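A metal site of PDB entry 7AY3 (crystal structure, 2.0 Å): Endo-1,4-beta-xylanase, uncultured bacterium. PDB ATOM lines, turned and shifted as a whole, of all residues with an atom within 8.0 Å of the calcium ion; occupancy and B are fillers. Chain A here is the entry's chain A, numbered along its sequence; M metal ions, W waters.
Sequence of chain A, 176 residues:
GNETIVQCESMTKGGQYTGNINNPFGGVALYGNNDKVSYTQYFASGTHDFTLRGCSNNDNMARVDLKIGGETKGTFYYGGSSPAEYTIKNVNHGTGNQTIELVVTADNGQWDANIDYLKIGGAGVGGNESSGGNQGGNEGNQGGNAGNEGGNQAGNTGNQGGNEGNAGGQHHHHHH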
ATOM      1  N   LEU A  30     -19.747   2.679   9.154  1.00  0.00           N
ATOM      2  CA  LEU A  30     -19.179   1.841  10.216  1.00  0.00           C
ATOM      3  C   LEU A  30     -19.663   0.424   9.960  1.00  0.00           C
ATOM      4  O   LEU A  30     -20.863   0.149  10.033  1.00  0.00           O
ATOM      5  CB  LEU A  30     -19.605   2.324  11.601  1.00  0.00           C
ATOM      6  CG  LEU A  30     -19.509   3.830  11.851  1.00  0.00           C
ATOM      7  CD1 LEU A  30     -20.001   4.164  13.259  1.00  0.00           C
ATOM      8  CD2 LEU A  30     -18.081   4.312  11.654  1.00  0.00           C
ATOM      9  N   TYR A  31     -18.718  -0.475   9.647  1.00  0.00           N
ATOM     10  CA  TYR A  31     -19.009  -1.815   9.163  1.00  0.00           C
ATOM     11  C   TYR A  31     -18.986  -2.879  10.236  1.00  0.00           C
ATOM     12  O   TYR A  31     -19.597  -3.936  10.059  1.00  0.00           O
ATOM     13  CB  TYR A  31     -18.009  -2.208   8.075  1.00  0.00           C
ATOM     14  CG  TYR A  31     -18.049  -1.326   6.841  1.00  0.00           C
ATOM     15  CD1 TYR A  31     -18.976  -1.565   5.831  1.00  0.00           C
ATOM     16  CD2 TYR A  31     -17.159  -0.270   6.673  1.00  0.00           C
ATOM     17  CE1 TYR A  31     -19.016  -0.773   4.698  1.00  0.00           C
ATOM     18  CE2 TYR A  31     -17.183   0.523   5.533  1.00  0.00           C
ATOM     19  CZ  TYR A  31     -18.122   0.275   4.550  1.00  0.00           C
ATOM     20  OH  TYR A  31     -18.178   1.042   3.419  1.00  0.00           O
ATOM     21  N   GLY A  32     -18.269  -2.662  11.342  1.00  0.00           N
ATOM     22  CA  GLY A  32     -18.192  -3.690  12.342  1.00  0.00           C
ATOM     23  C   GLY A  32     -17.952  -3.094  13.712  1.00  0.00           C
ATOM     24  O   GLY A  32     -17.829  -1.885  13.884  1.00  0.00           O
ATOM     25  N   ASN A  33     -17.887  -3.979  14.698  1.00  0.00           N
ATOM     26  CA  ASN A  33     -17.724  -3.528  16.065  1.00  0.00           C
ATOM     27  C   ASN A  33     -16.395  -2.807  16.226  1.00  0.00           C
ATOM     28  O   ASN A  33     -15.366  -3.231  15.685  1.00  0.00           O
ATOM     29  CB  ASN A  33     -17.836  -4.711  17.010  1.00  0.00           C
ATOM     30  CG  ASN A  33     -19.253  -5.209  17.096  1.00  0.00           C
ATOM     31  OD1 ASN A  33     -20.209  -4.454  16.844  1.00  0.00           O
ATOM     32  ND2 ASN A  33     -19.424  -6.465  17.448  1.00  0.00           N
ATOM     33  N   ASP A  35     -15.630  -0.072  14.875  1.00  0.00           N
ATOM     34  CA  ASP A  35     -15.552   0.968  13.855  1.00  0.00           C
ATOM     35  C   ASP A  35     -16.154   2.247  14.435  1.00  0.00           C
ATOM     36  O   ASP A  35     -17.255   2.245  14.965  1.00  0.00           O
ATOM     37  CB  ASP A  35     -16.321   0.557  12.593  1.00  0.00           C
ATOM     38  CG  ASP A  35     -15.478  -0.302  11.641  1.00  0.00           C
ATOM     39  OD1 ASP A  35     -14.354  -0.709  11.981  1.00  0.00           O
ATOM     40  OD2 ASP A  35     -15.971  -0.567  10.520  1.00  0.00           O
ATOM     41  N   ASN A  57     -27.736   0.326   6.031  1.00  0.00           N
ATOM     42  CA  ASN A  57     -27.595   0.015   4.618  1.00  0.00           C
ATOM     43  C   ASN A  57     -28.752  -0.816   4.076  1.00  0.00           C
ATOM     44  O   ASN A  57     -28.841  -0.988   2.856  1.00  0.00           O
ATOM     45  CB  ASN A  57     -26.266  -0.726   4.362  1.00  0.00           C
ATOM     46  CG  ASN A  57     -26.254  -2.105   5.001  1.00  0.00           C
ATOM     47  OD1 ASN A  57     -26.748  -2.279   6.107  1.00  0.00           O
ATOM     48  ND2 ASN A  57     -25.707  -3.081   4.292  1.00  0.00           N
ATOM     49  N   VAL A 104     -19.846   1.733  16.555  1.00  0.00           N
ATOM     50  CA  VAL A 104     -20.686   0.545  16.478  1.00  0.00           C
ATOM     51  C   VAL A 104     -20.196  -0.473  17.501  1.00  0.00           C
ATOM     52  O   VAL A 104     -18.990  -0.725  17.622  1.00  0.00           O
ATOM     53  CB  VAL A 104     -20.686  -0.060  15.063  1.00  0.00           C
ATOM     54  CG1 VAL A 104     -21.216  -1.487  15.078  1.00  0.00           C
ATOM     55  CG2 VAL A 104     -21.537   0.786  14.121  1.00  0.00           C
ATOM     56  N   ALA A 106     -22.887  -3.132  18.302  1.00  0.00           N
ATOM     57  CA  ALA A 106     -23.939  -4.129  18.208  1.00  0.00           C
ATOM     58  C   ALA A 106     -23.975  -4.809  16.842  1.00  0.00           C
ATOM     59  O   ALA A 106     -25.014  -5.339  16.439  1.00  0.00           O
ATOM     60  CB  ALA A 106     -25.298  -3.495  18.504  1.00  0.00           C
ATOM     61  N   ASP A 107     -22.863  -4.819  16.116  1.00  0.00           N
ATOM     62  CA  ASP A 107     -22.847  -5.441  14.809  1.00  0.00           C
ATOM     63  C   ASP A 107     -22.930  -6.957  14.936  1.00  0.00           C
ATOM     64  O   ASP A 107     -22.388  -7.563  15.866  1.00  0.00           O
ATOM     65  CB  ASP A 107     -21.594  -5.038  14.030  1.00  0.00           C
ATOM     66  CG  ASP A 107     -21.488  -5.735  12.683  1.00  0.00           C
ATOM     67  OD1 ASP A 107     -22.300  -5.463  11.785  1.00  0.00           O
ATOM     68  OD2 ASP A 107     -20.572  -6.572  12.521  1.00  0.00           O
ATOM     69  N   ASN A 108     -23.677  -7.581  14.024  1.00  0.00           N
ATOM     70  CA  ASN A 108     -23.735  -9.037  13.987  1.00  0.00           C
ATOM     71  C   ASN A 108     -23.803  -9.534  12.553  1.00  0.00           C
ATOM     72  O   ASN A 108     -24.410 -10.582  12.282  1.00  0.00           O
ATOM     73  CB  ASN A 108     -24.906  -9.567  14.815  1.00  0.00           C
ATOM     74  CG  ASN A 108     -26.250  -9.234  14.213  1.00  0.00           C
ATOM     75  OD1 ASN A 108     -26.397  -8.273  13.435  1.00  0.00           O
ATOM     76  ND2 ASN A 108     -27.270 -10.021  14.585  1.00  0.00           N
ATOM     77  N   GLY A 109     -23.196  -8.792  11.624  1.00  0.00           N
ATOM     78  CA  GLY A 109     -23.086  -9.191  10.240  1.00  0.00           C
ATOM     79  C   GLY A 109     -24.308  -8.953   9.392  1.00  0.00           C
ATOM     80  O   GLY A 109     -24.321  -9.378   8.230  1.00  0.00           O
ATOM     81  N   GLN A 110     -25.335  -8.275   9.926  1.00  0.00           N
ATOM     82  CA  GLN A 110     -26.604  -8.095   9.237  1.00  0.00           C
ATOM     83  C   GLN A 110     -26.838  -6.681   8.720  1.00  0.00           C
ATOM     84  O   GLN A 110     -27.753  -6.472   7.934  1.00  0.00           O
ATOM     85  CB  GLN A 110     -27.772  -8.479  10.171  1.00  0.00           C
ATOM     86  CG  GLN A 110     -27.678  -9.913  10.668  1.00  0.00           C
ATOM     87  CD  GLN A 110     -27.465 -10.936   9.541  1.00  0.00           C
ATOM     88  OE1 GLN A 110     -26.358 -11.432   9.329  1.00  0.00           O
ATOM     89  NE2 GLN A 110     -28.533 -11.246   8.817  1.00  0.00           N
ATOM     90  N   TRP A 111     -26.029  -5.713   9.137  1.00  0.00           N
ATOM     91  CA  TRP A 111     -26.208  -4.344   8.681  1.00  0.00           C
ATOM     92  C   TRP A 111     -24.912  -3.578   8.889  1.00  0.00           C
ATOM     93  O   TRP A 111     -24.039  -3.985   9.671  1.00  0.00           O
ATOM     94  CB  TRP A 111     -27.350  -3.650   9.419  1.00  0.00           C
ATOM     95  CG  TRP A 111     -27.253  -3.822  10.915  1.00  0.00           C
ATOM     96  CD1 TRP A 111     -27.931  -4.727  11.678  1.00  0.00           C
ATOM     97  CD2 TRP A 111     -26.435  -3.070  11.828  1.00  0.00           C
ATOM     98  NE1 TRP A 111     -27.574  -4.604  12.998  1.00  0.00           N
ATOM     99  CE2 TRP A 111     -26.674  -3.584  13.125  1.00  0.00           C
ATOM    100  CE3 TRP A 111     -25.541  -1.998  11.685  1.00  0.00           C
ATOM    101  CZ2 TRP A 111     -26.047  -3.067  14.267  1.00  0.00           C
ATOM    102  CZ3 TRP A 111     -24.896  -1.497  12.808  1.00  0.00           C
ATOM    103  CH2 TRP A 111     -25.163  -2.032  14.081  1.00  0.00           C
ATOM    104  N   ASP A 112     -24.808  -2.452   8.180  1.00  0.00           N
ATOM    105  CA  ASP A 112     -23.783  -1.446   8.375  1.00  0.00           C
ATOM    106  C   ASP A 112     -24.470  -0.135   8.747  1.00  0.00           C
ATOM    107  O   ASP A 112     -25.624   0.106   8.380  1.00  0.00           O
ATOM    108  CB  ASP A 112     -22.932  -1.242   7.123  1.00  0.00           C
ATOM    109  CG  ASP A 112     -22.242  -2.514   6.678  1.00  0.00           C
ATOM    110  OD1 ASP A 112     -21.850  -3.293   7.563  1.00  0.00           O
ATOM    111  OD2 ASP A 112     -22.085  -2.735   5.449  1.00  0.00           O
ATOM    112  N   ALA A 113     -23.765   0.725   9.473  1.00  0.00           N
ATOM    113  CA  ALA A 113     -24.302   2.022   9.870  1.00  0.00           C
ATOM    114  C   ALA A 113     -23.662   3.109   9.009  1.00  0.00           C
ATOM    115  O   ALA A 113     -22.433   3.227   8.972  1.00  0.00           O
ATOM    116  CB  ALA A 113     -24.033   2.281  11.349  1.00  0.00           C
HETATM  117 CA    CA M   1     -21.726  -4.513   9.559  1.00  0.00          CA
HETATM  118  O   HOH W   1     -21.753  -2.177  11.550  1.00  0.00           O
HETATM  119  O   HOH W   2     -19.985  -5.370   7.327  1.00  0.00           O
HETATM  120  O   HOH W   3     -22.655  -6.309   7.847  1.00  0.00           O
HETATM  121  O   HOH W   4     -20.639  -6.796   9.732  1.00  0.00           O
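The calcium ion is bound by the backbone carbonyl oxygen (O) of Tyr 31 (2.3 Å), the side-chain carboxylate (OD1) of Asp 112 (2.3 Å), the backbone carbonyl oxygen (O) of Trp 111 (2.4 Å), the side-chain carboxylate (OD1) of Asp 107 (2.5 Å), water W4 (2.5 Å) and water W3 (2.6 Å).
The calcium ion has six donor atoms within binding distance.
Slightly farther from the calcium ion lies water W2 (3.0 Å).
Slightly farther from the calcium ion lies water W1 (3.1 Å).
N of Tyr 31 is in hydrogen-bond range of OD2 of Asp 35 (2.9 Å).
The side-chain amide oxygen of Asn 57 sits at hydrogen-bond distance from the backbone NH of Asp 112 (2.8 Å).
The side-chain carboxylate (OD1) of Asp 107 lies close to the backbone NH (N) of Gly 109, 3.5 Å away.
The side-chain amide oxygen (OD1) of Asn 33 sits at hydrogen-bond distance from the backbone NH (N) of Asp 107 (2.8 Å).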
